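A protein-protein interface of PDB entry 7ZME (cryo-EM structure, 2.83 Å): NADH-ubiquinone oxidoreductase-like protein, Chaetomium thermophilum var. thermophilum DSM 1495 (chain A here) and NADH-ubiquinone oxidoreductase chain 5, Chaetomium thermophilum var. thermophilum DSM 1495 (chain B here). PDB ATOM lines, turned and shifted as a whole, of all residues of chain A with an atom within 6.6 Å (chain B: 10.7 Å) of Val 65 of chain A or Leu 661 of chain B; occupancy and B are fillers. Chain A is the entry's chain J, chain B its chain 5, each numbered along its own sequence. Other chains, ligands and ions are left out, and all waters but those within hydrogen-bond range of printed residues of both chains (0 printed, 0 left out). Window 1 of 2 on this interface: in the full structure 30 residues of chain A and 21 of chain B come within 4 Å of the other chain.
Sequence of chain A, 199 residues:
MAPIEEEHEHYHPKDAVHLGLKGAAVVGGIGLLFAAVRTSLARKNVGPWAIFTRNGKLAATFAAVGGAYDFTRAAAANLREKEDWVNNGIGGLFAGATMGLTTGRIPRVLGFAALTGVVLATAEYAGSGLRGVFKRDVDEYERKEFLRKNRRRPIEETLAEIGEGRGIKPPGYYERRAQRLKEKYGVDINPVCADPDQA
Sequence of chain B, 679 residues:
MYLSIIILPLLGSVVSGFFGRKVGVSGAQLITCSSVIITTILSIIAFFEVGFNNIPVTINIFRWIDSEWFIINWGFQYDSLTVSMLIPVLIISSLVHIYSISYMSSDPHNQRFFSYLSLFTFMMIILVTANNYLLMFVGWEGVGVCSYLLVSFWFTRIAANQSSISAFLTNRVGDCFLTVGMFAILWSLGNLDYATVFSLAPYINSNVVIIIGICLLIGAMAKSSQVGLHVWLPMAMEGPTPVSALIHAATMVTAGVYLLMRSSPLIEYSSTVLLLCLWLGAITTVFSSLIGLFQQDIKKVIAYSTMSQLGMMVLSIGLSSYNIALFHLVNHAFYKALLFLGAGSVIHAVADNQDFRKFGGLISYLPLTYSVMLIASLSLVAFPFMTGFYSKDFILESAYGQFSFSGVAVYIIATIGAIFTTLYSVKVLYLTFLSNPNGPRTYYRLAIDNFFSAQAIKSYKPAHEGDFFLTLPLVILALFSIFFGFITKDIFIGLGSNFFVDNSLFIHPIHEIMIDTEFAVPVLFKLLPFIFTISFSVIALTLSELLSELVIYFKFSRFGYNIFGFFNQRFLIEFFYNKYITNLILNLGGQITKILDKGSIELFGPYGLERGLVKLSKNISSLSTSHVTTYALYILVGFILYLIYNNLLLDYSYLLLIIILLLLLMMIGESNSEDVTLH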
ATOM      1  N   GLY A  23     -18.228  -2.657  -6.037  1.00  0.00           N
ATOM      2  CA  GLY A  23     -17.511  -2.707  -7.301  1.00  0.00           C
ATOM      3  C   GLY A  23     -17.391  -1.346  -7.957  1.00  0.00           C
ATOM      4  O   GLY A  23     -16.358  -1.020  -8.549  1.00  0.00           O
ATOM      5  N   ALA A  24     -18.446  -0.536  -7.871  1.00  0.00           N
ATOM      6  CA  ALA A  24     -18.385   0.817  -8.412  1.00  0.00           C
ATOM      7  C   ALA A  24     -17.393   1.676  -7.639  1.00  0.00           C
ATOM      8  O   ALA A  24     -16.651   2.466  -8.233  1.00  0.00           O
ATOM      9  CB  ALA A  24     -19.774   1.453  -8.395  1.00  0.00           C
ATOM     10  N   VAL A  27     -13.572   0.387  -8.597  1.00  0.00           N
ATOM     11  CA  VAL A  27     -13.194   0.766  -9.954  1.00  0.00           C
ATOM     12  C   VAL A  27     -13.296   2.273 -10.136  1.00  0.00           C
ATOM     13  O   VAL A  27     -12.423   2.897 -10.747  1.00  0.00           O
ATOM     14  CB  VAL A  27     -14.060   0.010 -10.977  1.00  0.00           C
ATOM     15  CG1 VAL A  27     -13.759   0.493 -12.377  1.00  0.00           C
ATOM     16  CG2 VAL A  27     -13.828  -1.484 -10.867  1.00  0.00           C
ATOM     17  N   ALA A  60     -16.989   9.133 -13.136  1.00  0.00           N
ATOM     18  CA  ALA A  60     -18.353   8.640 -13.293  1.00  0.00           C
ATOM     19  C   ALA A  60     -18.403   7.489 -14.284  1.00  0.00           C
ATOM     20  O   ALA A  60     -19.137   6.515 -14.082  1.00  0.00           O
ATOM     21  CB  ALA A  60     -19.278   9.773 -13.735  1.00  0.00           C
ATOM     22  N   THR A  61     -17.632   7.586 -15.368  1.00  0.00           N
ATOM     23  CA  THR A  61     -17.567   6.488 -16.325  1.00  0.00           C
ATOM     24  C   THR A  61     -16.988   5.238 -15.686  1.00  0.00           C
ATOM     25  O   THR A  61     -17.472   4.128 -15.928  1.00  0.00           O
ATOM     26  CB  THR A  61     -16.739   6.890 -17.547  1.00  0.00           C
ATOM     27  OG1 THR A  61     -17.284   8.085 -18.120  1.00  0.00           O
ATOM     28  CG2 THR A  61     -16.742   5.782 -18.594  1.00  0.00           C
ATOM     29  N   PHE A  62     -15.954   5.392 -14.862  1.00  0.00           N
ATOM     30  CA  PHE A  62     -15.267   4.203 -14.384  1.00  0.00           C
ATOM     31  C   PHE A  62     -16.115   3.486 -13.343  1.00  0.00           C
ATOM     32  O   PHE A  62     -16.198   2.253 -13.337  1.00  0.00           O
ATOM     33  CB  PHE A  62     -13.916   4.560 -13.773  1.00  0.00           C
ATOM     34  CG  PHE A  62     -12.824   4.746 -14.783  1.00  0.00           C
ATOM     35  CD1 PHE A  62     -13.103   4.713 -16.130  1.00  0.00           C
ATOM     36  CD2 PHE A  62     -11.500   4.822 -14.387  1.00  0.00           C
ATOM     37  CE1 PHE A  62     -12.105   4.895 -17.047  1.00  0.00           C
ATOM     38  CE2 PHE A  62     -10.489   4.977 -15.295  1.00  0.00           C
ATOM     39  CZ  PHE A  62     -10.789   5.002 -16.623  1.00  0.00           C
ATOM     40  N   ALA A  63     -16.739   4.250 -12.444  1.00  0.00           N
ATOM     41  CA  ALA A  63     -17.630   3.662 -11.453  1.00  0.00           C
ATOM     42  C   ALA A  63     -18.875   3.076 -12.099  1.00  0.00           C
ATOM     43  O   ALA A  63     -19.469   2.137 -11.559  1.00  0.00           O
ATOM     44  CB  ALA A  63     -18.020   4.712 -10.413  1.00  0.00           C
ATOM     45  N   ALA A  64     -19.296   3.627 -13.236  1.00  0.00           N
ATOM     46  CA  ALA A  64     -20.429   3.053 -13.949  1.00  0.00           C
ATOM     47  C   ALA A  64     -20.113   1.642 -14.425  1.00  0.00           C
ATOM     48  O   ALA A  64     -20.969   0.753 -14.362  1.00  0.00           O
ATOM     49  CB  ALA A  64     -20.817   3.948 -15.125  1.00  0.00           C
ATOM     50  N   VAL A  65     -18.888   1.418 -14.899  1.00  0.00           N
ATOM     51  CA  VAL A  65     -18.498   0.091 -15.359  1.00  0.00           C
ATOM     52  C   VAL A  65     -18.341  -0.862 -14.185  1.00  0.00           C
ATOM     53  O   VAL A  65     -18.732  -2.032 -14.261  1.00  0.00           O
ATOM     54  CB  VAL A  65     -17.204   0.175 -16.187  1.00  0.00           C
ATOM     55  CG1 VAL A  65     -16.875  -1.181 -16.787  1.00  0.00           C
ATOM     56  CG2 VAL A  65     -17.327   1.243 -17.244  1.00  0.00           C
ATOM     57  N   GLY A  66     -17.751  -0.385 -13.088  1.00  0.00           N
ATOM     58  CA  GLY A  66     -17.543  -1.250 -11.939  1.00  0.00           C
ATOM     59  C   GLY A  66     -18.844  -1.739 -11.339  1.00  0.00           C
ATOM     60  O   GLY A  66     -18.989  -2.923 -11.026  1.00  0.00           O
ATOM     61  N   GLY A  67     -19.808  -0.836 -11.171  1.00  0.00           N
ATOM     62  CA  GLY A  67     -21.120  -1.257 -10.715  1.00  0.00           C
ATOM     63  C   GLY A  67     -21.828  -2.132 -11.730  1.00  0.00           C
ATOM     64  O   GLY A  67     -22.481  -3.112 -11.367  1.00  0.00           O
ATOM     65  N   ALA A  68     -21.707  -1.793 -13.016  1.00  0.00           N
ATOM     66  CA  ALA A  68     -22.339  -2.602 -14.052  1.00  0.00           C
ATOM     67  C   ALA A  68     -21.719  -3.989 -14.128  1.00  0.00           C
ATOM     68  O   ALA A  68     -22.422  -4.974 -14.377  1.00  0.00           O
ATOM     69  CB  ALA A  68     -22.242  -1.900 -15.406  1.00  0.00           C
ATOM     70  N   TYR A  69     -20.403  -4.090 -13.931  1.00  0.00           N
ATOM     71  CA  TYR A  69     -19.770  -5.402 -13.935  1.00  0.00           C
ATOM     72  C   TYR A  69     -20.118  -6.193 -12.684  1.00  0.00           C
ATOM     73  O   TYR A  69     -20.444  -7.379 -12.769  1.00  0.00           O
ATOM     74  CB  TYR A  69     -18.254  -5.276 -14.061  1.00  0.00           C
ATOM     75  CG  TYR A  69     -17.543  -6.599 -13.889  1.00  0.00           C
ATOM     76  CD1 TYR A  69     -17.923  -7.711 -14.622  1.00  0.00           C
ATOM     77  CD2 TYR A  69     -16.505  -6.742 -12.982  1.00  0.00           C
ATOM     78  CE1 TYR A  69     -17.290  -8.923 -14.465  1.00  0.00           C
ATOM     79  CE2 TYR A  69     -15.864  -7.953 -12.820  1.00  0.00           C
ATOM     80  CZ  TYR A  69     -16.262  -9.037 -13.565  1.00  0.00           C
ATOM     81  OH  TYR A  69     -15.626 -10.243 -13.410  1.00  0.00           O
ATOM     82  N   ASP A  70     -20.049  -5.559 -11.516  1.00  0.00           N
ATOM     83  CA  ASP A  70     -20.189  -6.316 -10.278  1.00  0.00           C
ATOM     84  C   ASP A  70     -21.641  -6.701 -10.027  1.00  0.00           C
ATOM     85  O   ASP A  70     -21.924  -7.822  -9.591  1.00  0.00           O
ATOM     86  CB  ASP A  70     -19.620  -5.513  -9.108  1.00  0.00           C
ATOM     87  CG  ASP A  70     -19.398  -6.360  -7.868  1.00  0.00           C
ATOM     88  OD1 ASP A  70     -19.717  -7.566  -7.896  1.00  0.00           O
ATOM     89  OD2 ASP A  70     -18.879  -5.821  -6.869  1.00  0.00           O
ATOM     90  N   GLY A  91     -21.282 -10.522 -16.710  1.00  0.00           N
ATOM     91  CA  GLY A  91     -20.804  -9.264 -16.165  1.00  0.00           C
ATOM     92  C   GLY A  91     -19.866  -8.546 -17.114  1.00  0.00           C
ATOM     93  O   GLY A  91     -19.858  -7.315 -17.181  1.00  0.00           O
ATOM     94  N   PHE A  94     -22.089  -6.892 -19.844  1.00  0.00           N
ATOM     95  CA  PHE A  94     -22.749  -5.684 -19.372  1.00  0.00           C
ATOM     96  C   PHE A  94     -21.753  -4.596 -18.997  1.00  0.00           C
ATOM     97  O   PHE A  94     -22.069  -3.408 -19.119  1.00  0.00           O
ATOM     98  CB  PHE A  94     -23.663  -6.013 -18.194  1.00  0.00           C
ATOM     99  CG  PHE A  94     -24.950  -6.672 -18.599  1.00  0.00           C
ATOM    100  CD1 PHE A  94     -25.938  -5.948 -19.244  1.00  0.00           C
ATOM    101  CD2 PHE A  94     -25.168  -8.014 -18.346  1.00  0.00           C
ATOM    102  CE1 PHE A  94     -27.122  -6.548 -19.623  1.00  0.00           C
ATOM    103  CE2 PHE A  94     -26.351  -8.621 -18.724  1.00  0.00           C
ATOM    104  CZ  PHE A  94     -27.327  -7.887 -19.363  1.00  0.00           C
ATOM    105  N   ALA A  95     -20.565  -4.971 -18.524  1.00  0.00           N
ATOM    106  CA  ALA A  95     -19.500  -3.987 -18.379  1.00  0.00           C
ATOM    107  C   ALA A  95     -19.067  -3.456 -19.735  1.00  0.00           C
ATOM    108  O   ALA A  95     -18.865  -2.250 -19.903  1.00  0.00           O
ATOM    109  CB  ALA A  95     -18.310  -4.593 -17.638  1.00  0.00           C
ATOM    110  N   GLY A  96     -18.915  -4.345 -20.715  1.00  0.00           N
ATOM    111  CA  GLY A  96     -18.602  -3.897 -22.059  1.00  0.00           C
ATOM    112  C   GLY A  96     -19.725  -3.087 -22.669  1.00  0.00           C
ATOM    113  O   GLY A  96     -19.484  -2.067 -23.321  1.00  0.00           O
ATOM    114  N   THR A  98     -21.954  -1.232 -21.121  1.00  0.00           N
ATOM    115  CA  THR A  98     -22.080   0.084 -20.506  1.00  0.00           C
ATOM    116  C   THR A  98     -20.949   1.008 -20.943  1.00  0.00           C
ATOM    117  O   THR A  98     -21.107   2.233 -20.953  1.00  0.00           O
ATOM    118  CB  THR A  98     -22.136  -0.038 -18.980  1.00  0.00           C
ATOM    119  OG1 THR A  98     -22.640   1.182 -18.422  1.00  0.00           O
ATOM    120  CG2 THR A  98     -20.762  -0.314 -18.396  1.00  0.00           C
ATOM    121  N   MET A  99     -19.798   0.441 -21.315  1.00  0.00           N
ATOM    122  CA  MET A  99     -18.733   1.269 -21.868  1.00  0.00           C
ATOM    123  C   MET A  99     -19.088   1.755 -23.265  1.00  0.00           C
ATOM    124  O   MET A  99     -18.567   2.776 -23.728  1.00  0.00           O
ATOM    125  CB  MET A  99     -17.407   0.508 -21.870  1.00  0.00           C
ATOM    126  CG  MET A  99     -16.888   0.223 -20.473  1.00  0.00           C
ATOM    127  SD  MET A  99     -15.294  -0.613 -20.353  1.00  0.00           S
ATOM    128  CE  MET A  99     -15.733  -2.279 -20.819  1.00  0.00           C
ATOM    129  N   THR A 116     -14.852  -7.298 -23.709  1.00  0.00           N
ATOM    130  CA  THR A 116     -14.711  -7.417 -22.262  1.00  0.00           C
ATOM    131  C   THR A 116     -15.274  -8.735 -21.753  1.00  0.00           C
ATOM    132  O   THR A 116     -14.735  -9.324 -20.810  1.00  0.00           O
ATOM    133  CB  THR A 116     -15.399  -6.241 -21.575  1.00  0.00           C
ATOM    134  OG1 THR A 116     -15.100  -5.036 -22.288  1.00  0.00           O
ATOM    135  CG2 THR A 116     -14.922  -6.108 -20.139  1.00  0.00           C
ATOM    136  N   LEU B 616      -5.403   3.388 -32.068  1.00  0.00           N
ATOM    137  CA  LEU B 616      -5.044   3.172 -30.670  1.00  0.00           C
ATOM    138  C   LEU B 616      -3.571   3.461 -30.420  1.00  0.00           C
ATOM    139  O   LEU B 616      -3.215   4.087 -29.416  1.00  0.00           O
ATOM    140  CB  LEU B 616      -5.382   1.741 -30.259  1.00  0.00           C
ATOM    141  CG  LEU B 616      -4.964   1.327 -28.848  1.00  0.00           C
ATOM    142  CD1 LEU B 616      -5.740   2.118 -27.826  1.00  0.00           C
ATOM    143  CD2 LEU B 616      -5.162  -0.157 -28.635  1.00  0.00           C
ATOM    144  N   LEU B 641      -0.653   2.520  -8.187  1.00  0.00           N
ATOM    145  CA  LEU B 641      -1.638   1.560  -8.674  1.00  0.00           C
ATOM    146  C   LEU B 641      -1.232   0.131  -8.339  1.00  0.00           C
ATOM    147  O   LEU B 641      -2.087  -0.704  -8.026  1.00  0.00           O
ATOM    148  CB  LEU B 641      -1.831   1.725 -10.179  1.00  0.00           C
ATOM    149  CG  LEU B 641      -3.003   2.595 -10.634  1.00  0.00           C
ATOM    150  CD1 LEU B 641      -2.998   2.738 -12.136  1.00  0.00           C
ATOM    151  CD2 LEU B 641      -4.325   2.033 -10.152  1.00  0.00           C
ATOM    152  N   SER B 653     -10.159  -9.804 -11.831  1.00  0.00           N
ATOM    153  CA  SER B 653     -11.097  -9.344 -12.848  1.00  0.00           C
ATOM    154  C   SER B 653     -11.116  -7.825 -12.920  1.00  0.00           C
ATOM    155  O   SER B 653     -11.191  -7.247 -14.010  1.00  0.00           O
ATOM    156  CB  SER B 653     -12.494  -9.881 -12.550  1.00  0.00           C
ATOM    157  OG  SER B 653     -13.025  -9.257 -11.398  1.00  0.00           O
ATOM    158  N   TYR B 654     -11.061  -7.164 -11.762  1.00  0.00           N
ATOM    159  CA  TYR B 654     -10.981  -5.709 -11.736  1.00  0.00           C
ATOM    160  C   TYR B 654      -9.775  -5.214 -12.518  1.00  0.00           C
ATOM    161  O   TYR B 654      -9.886  -4.294 -13.333  1.00  0.00           O
ATOM    162  CB  TYR B 654     -10.921  -5.218 -10.291  1.00  0.00           C
ATOM    163  CG  TYR B 654     -12.175  -5.488  -9.499  1.00  0.00           C
ATOM    164  CD1 TYR B 654     -13.426  -5.168 -10.012  1.00  0.00           C
ATOM    165  CD2 TYR B 654     -12.113  -6.051  -8.234  1.00  0.00           C
ATOM    166  CE1 TYR B 654     -14.578  -5.410  -9.292  1.00  0.00           C
ATOM    167  CE2 TYR B 654     -13.261  -6.296  -7.505  1.00  0.00           C
ATOM    168  CZ  TYR B 654     -14.491  -5.973  -8.038  1.00  0.00           C
ATOM    169  OH  TYR B 654     -15.635  -6.216  -7.315  1.00  0.00           O
ATOM    170  N   LEU B 655      -8.611  -5.827 -12.291  1.00  0.00           N
ATOM    171  CA  LEU B 655      -7.410  -5.417 -13.011  1.00  0.00           C
ATOM    172  C   LEU B 655      -7.560  -5.624 -14.511  1.00  0.00           C
ATOM    173  O   LEU B 655      -7.195  -4.749 -15.302  1.00  0.00           O
ATOM    174  CB  LEU B 655      -6.195  -6.167 -12.463  1.00  0.00           C
ATOM    175  CG  LEU B 655      -4.827  -5.654 -12.909  1.00  0.00           C
ATOM    176  CD1 LEU B 655      -3.835  -5.740 -11.790  1.00  0.00           C
ATOM    177  CD2 LEU B 655      -4.340  -6.514 -14.052  1.00  0.00           C
ATOM    178  N   LEU B 656      -8.099  -6.770 -14.926  1.00  0.00           N
ATOM    179  CA  LEU B 656      -8.386  -6.965 -16.342  1.00  0.00           C
ATOM    180  C   LEU B 656      -9.432  -5.973 -16.831  1.00  0.00           C
ATOM    181  O   LEU B 656      -9.328  -5.451 -17.947  1.00  0.00           O
ATOM    182  CB  LEU B 656      -8.848  -8.394 -16.599  1.00  0.00           C
ATOM    183  CG  LEU B 656      -7.734  -9.413 -16.804  1.00  0.00           C
ATOM    184  CD1 LEU B 656      -8.327 -10.787 -16.985  1.00  0.00           C
ATOM    185  CD2 LEU B 656      -6.879  -9.036 -18.000  1.00  0.00           C
ATOM    186  N   LEU B 657     -10.444  -5.698 -16.010  1.00  0.00           N
ATOM    187  CA  LEU B 657     -11.464  -4.734 -16.402  1.00  0.00           C
ATOM    188  C   LEU B 657     -10.863  -3.353 -16.615  1.00  0.00           C
ATOM    189  O   LEU B 657     -11.176  -2.685 -17.603  1.00  0.00           O
ATOM    190  CB  LEU B 657     -12.573  -4.680 -15.353  1.00  0.00           C
ATOM    191  CG  LEU B 657     -13.735  -3.748 -15.690  1.00  0.00           C
ATOM    192  CD1 LEU B 657     -14.432  -4.221 -16.946  1.00  0.00           C
ATOM    193  CD2 LEU B 657     -14.711  -3.670 -14.532  1.00  0.00           C
ATOM    194  N   ILE B 658      -9.978  -2.918 -15.713  1.00  0.00           N
ATOM    195  CA  ILE B 658      -9.341  -1.610 -15.860  1.00  0.00           C
ATOM    196  C   ILE B 658      -8.532  -1.543 -17.148  1.00  0.00           C
ATOM    197  O   ILE B 658      -8.577  -0.542 -17.872  1.00  0.00           O
ATOM    198  CB  ILE B 658      -8.463  -1.293 -14.636  1.00  0.00           C
ATOM    199  CG1 ILE B 658      -9.296  -1.294 -13.358  1.00  0.00           C
ATOM    200  CG2 ILE B 658      -7.778   0.048 -14.805  1.00  0.00           C
ATOM    201  CD1 ILE B 658     -10.392  -0.261 -13.351  1.00  0.00           C
ATOM    202  N   ILE B 659      -7.774  -2.599 -17.452  1.00  0.00           N
ATOM    203  CA  ILE B 659      -6.868  -2.554 -18.598  1.00  0.00           C
ATOM    204  C   ILE B 659      -7.649  -2.382 -19.893  1.00  0.00           C
ATOM    205  O   ILE B 659      -7.367  -1.477 -20.686  1.00  0.00           O
ATOM    206  CB  ILE B 659      -5.982  -3.811 -18.637  1.00  0.00           C
ATOM    207  CG1 ILE B 659      -4.945  -3.763 -17.521  1.00  0.00           C
ATOM    208  CG2 ILE B 659      -5.307  -3.947 -19.989  1.00  0.00           C
ATOM    209  CD1 ILE B 659      -4.367  -5.089 -17.211  1.00  0.00           C
ATOM    210  N   ILE B 660      -8.659  -3.225 -20.115  1.00  0.00           N
ATOM    211  CA  ILE B 660      -9.500  -3.071 -21.299  1.00  0.00           C
ATOM    212  C   ILE B 660     -10.133  -1.692 -21.301  1.00  0.00           C
ATOM    213  O   ILE B 660     -10.083  -0.956 -22.291  1.00  0.00           O
ATOM    214  CB  ILE B 660     -10.580  -4.164 -21.336  1.00  0.00           C
ATOM    215  CG1 ILE B 660      -9.959  -5.543 -21.178  1.00  0.00           C
ATOM    216  CG2 ILE B 660     -11.365  -4.078 -22.620  1.00  0.00           C
ATOM    217  CD1 ILE B 660     -10.928  -6.570 -20.675  1.00  0.00           C
ATOM    218  N   LEU B 661     -10.707  -1.321 -20.164  1.00  0.00           N
ATOM    219  CA  LEU B 661     -11.357  -0.032 -19.994  1.00  0.00           C
ATOM    220  C   LEU B 661     -10.419   1.136 -20.267  1.00  0.00           C
ATOM    221  O   LEU B 661     -10.873   2.199 -20.703  1.00  0.00           O
ATOM    222  CB  LEU B 661     -11.937  -0.009 -18.587  1.00  0.00           C
ATOM    223  CG  LEU B 661     -12.819   1.016 -17.934  1.00  0.00           C
ATOM    224  CD1 LEU B 661     -13.634   0.336 -16.886  1.00  0.00           C
ATOM    225  CD2 LEU B 661     -11.769   1.787 -17.231  1.00  0.00           C
ATOM    226  N   LEU B 662      -9.120   0.971 -20.017  1.00  0.00           N
ATOM    227  CA  LEU B 662      -8.175   2.021 -20.382  1.00  0.00           C
ATOM    228  C   LEU B 662      -7.892   2.023 -21.877  1.00  0.00           C
ATOM    229  O   LEU B 662      -7.694   3.089 -22.468  1.00  0.00           O
ATOM    230  CB  LEU B 662      -6.874   1.884 -19.591  1.00  0.00           C
ATOM    231  CG  LEU B 662      -6.944   2.186 -18.092  1.00  0.00           C
ATOM    232  CD1 LEU B 662      -5.722   1.649 -17.359  1.00  0.00           C
ATOM    233  CD2 LEU B 662      -7.097   3.677 -17.865  1.00  0.00           C
ATOM    234  N   LEU B 663      -7.860   0.846 -22.504  1.00  0.00           N
ATOM    235  CA  LEU B 663      -7.718   0.794 -23.953  1.00  0.00           C
ATOM    236  C   LEU B 663      -8.924   1.396 -24.653  1.00  0.00           C
ATOM    237  O   LEU B 663      -8.782   1.983 -25.731  1.00  0.00           O
ATOM    238  CB  LEU B 663      -7.506  -0.645 -24.415  1.00  0.00           C
ATOM    239  CG  LEU B 663      -6.498  -1.488 -23.636  1.00  0.00           C
ATOM    240  CD1 LEU B 663      -6.467  -2.907 -24.172  1.00  0.00           C
ATOM    241  CD2 LEU B 663      -5.118  -0.860 -23.691  1.00  0.00           C
ATOM    242  N   LEU B 664     -10.114   1.261 -24.066  1.00  0.00           N
ATOM    243  CA  LEU B 664     -11.306   1.828 -24.683  1.00  0.00           C
ATOM    244  C   LEU B 664     -11.340   3.342 -24.553  1.00  0.00           C
ATOM    245  O   LEU B 664     -11.886   4.021 -25.428  1.00  0.00           O
ATOM    246  CB  LEU B 664     -12.565   1.209 -24.075  1.00  0.00           C
ATOM    247  CG  LEU B 664     -12.576  -0.312 -23.917  1.00  0.00           C
ATOM    248  CD1 LEU B 664     -13.967  -0.801 -23.599  1.00  0.00           C
ATOM    249  CD2 LEU B 664     -12.043  -1.006 -25.163  1.00  0.00           C
ATOM    250  N   LEU B 665     -10.780   3.892 -23.474  1.00  0.00           N
ATOM    251  CA  LEU B 665     -10.595   5.337 -23.416  1.00  0.00           C
ATOM    252  C   LEU B 665      -9.559   5.790 -24.426  1.00  0.00           C
ATOM    253  O   LEU B 665      -9.762   6.781 -25.135  1.00  0.00           O
ATOM    254  CB  LEU B 665     -10.152   5.777 -22.029  1.00  0.00           C
ATOM    255  CG  LEU B 665     -11.035   5.648 -20.806  1.00  0.00           C
ATOM    256  CD1 LEU B 665     -10.164   6.063 -19.660  1.00  0.00           C
ATOM    257  CD2 LEU B 665     -12.255   6.541 -20.911  1.00  0.00           C
ATOM    258  N   MET B 666      -8.433   5.086 -24.487  1.00  0.00           N
ATOM    259  CA  MET B 666      -7.369   5.458 -25.403  1.00  0.00           C
ATOM    260  C   MET B 666      -7.799   5.271 -26.848  1.00  0.00           C
ATOM    261  O   MET B 666      -7.322   5.993 -27.728  1.00  0.00           O
ATOM    262  CB  MET B 666      -6.125   4.632 -25.104  1.00  0.00           C
ATOM    263  CG  MET B 666      -4.918   5.034 -25.900  1.00  0.00           C
ATOM    264  SD  MET B 666      -4.325   6.643 -25.361  1.00  0.00           S
ATOM    265  CE  MET B 666      -3.721   6.228 -23.732  1.00  0.00           C
ATOM    266  N   MET B 667      -8.695   4.319 -27.103  1.00  0.00           N
ATOM    267  CA  MET B 667      -9.329   4.214 -28.410  1.00  0.00           C
ATOM    268  C   MET B 667     -10.186   5.438 -28.702  1.00  0.00           C
ATOM    269  O   MET B 667     -10.203   5.934 -29.834  1.00  0.00           O
ATOM    270  CB  MET B 667     -10.171   2.942 -28.479  1.00  0.00           C
ATOM    271  CG  MET B 667      -9.461   1.772 -29.131  1.00  0.00           C
ATOM    272  SD  MET B 667      -9.116   2.046 -30.877  1.00  0.00           S
ATOM    273  CE  MET B 667     -10.652   2.791 -31.421  1.00  0.00           C
ATOM    274  N   ILE B 668     -10.902   5.937 -27.691  1.00  0.00           N
ATOM    275  CA  ILE B 668     -11.675   7.157 -27.862  1.00  0.00           C
ATOM    276  C   ILE B 668     -10.726   8.335 -28.061  1.00  0.00           C
ATOM    277  O   ILE B 668      -9.729   8.493 -27.344  1.00  0.00           O
ATOM    278  CB  ILE B 668     -12.605   7.386 -26.659  1.00  0.00           C
ATOM    279  CG1 ILE B 668     -13.751   6.374 -26.681  1.00  0.00           C
ATOM    280  CG2 ILE B 668     -13.149   8.807 -26.652  1.00  0.00           C
ATOM    281  CD1 ILE B 668     -14.448   6.278 -28.019  1.00  0.00           C
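Val 65 of chain A touches just these residues of chain B: Leu 657 (3.9 Å) and Leu 661 (3.6 Å). Leu 661 of chain B touches three residues of chain A. Printed residues of chain B within 4 Å of Phe 62 of chain A: Leu 661 and Leu 665. No residue of chain B comes within 4 Å of Ala 63 of chain A. No residue of chain B comes within 4 Å of Ala 64 of chain A. No residue of chain B comes within 4 Å of Gly 67 of chain A. Printed residues of chain B within 4 Å of Ala 95 of chain A: Leu 657 (3.96 Å). Printed residues of chain B within 4 Å of Tyr 69 of chain A: Ser 653 and Leu 657. Printed residues of chain B within 4 Å of Met 99 of chain A: Leu 661 and Leu 664. Of the printed residues of chain A, Ser 653 of chain B touches Tyr 69 (3.3 Å). Printed residues of chain A within 4 Å of Leu 664 of chain B: Met 99. Of the printed residues of chain A, Ile 658 of chain B touches Val 27 (3.6 Å). Ala 60 of chain A touches none of the printed residues of chain B. The nearest printed residue of chain B that does not touch Thr 116 of chain A is Leu 664 of chain B (4.6 Å).
OH of Tyr 69 of chain A sits close to OG of Ser 653 of chain B (3.4 Å). OD2 of Asp 70 of chain A lies within hydrogen-bond range of OH of Tyr 654 of chain B.
Tyr 654 of chain B touches Gly 23 of chain A. Tyr 654 of chain B touches Val 27 of chain A. Phe 62 of chain A touches Leu 661 of chain B. Phe 62 of chain A touches Leu 665 of chain B (CZ to CD1, 3.3 Å). Leu 657 of chain B touches Val 65 of chain A (CD1 to CG1, 3.9 Å). Leu 661 of chain B touches Val 65 of chain A (CD1 to CG1, 3.6 Å). Tyr 69 of chain A touches Leu 657 of chain B. CD1 of Leu 664 of chain B touches SD of Met 99 of chain A, at 3.5 Å. Thr 116 of chain A touches Leu 657 of chain B (CG2 to CD1, 3.7 Å). Thr 116 of chain A touches Ile 660 of chain B.
Of the 21 printed residues of chain A, 9 touch a printed residue of chain B. Hydrophobic or aromatic side chains of chain A that line the printed part of chain B: Val 27, Phe 62, Val 65, Tyr 69, Ala 95 and Met 99. Along chain A the printed residues that touch a printed residue of chain B span positions 23 to 116. Hydrophobic or aromatic side chains of chain B within 4 Å of the printed part of chain A: Tyr 654, Leu 657, Ile 658, Ile 660, Leu 661, Leu 664 and Leu 665. Among the printed residues, 15 pairs touch across the chains. Among the printed residues, no Asp or Glu carboxylate lies within 4 Å of a Lys or Arg side-chain nitrogen of the other chain.
The side-chain carboxylate of Asp 70 of chain A lies within hydrogen-bond range of the backbone NH of Gly 23 of chain A (3.3 Å).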
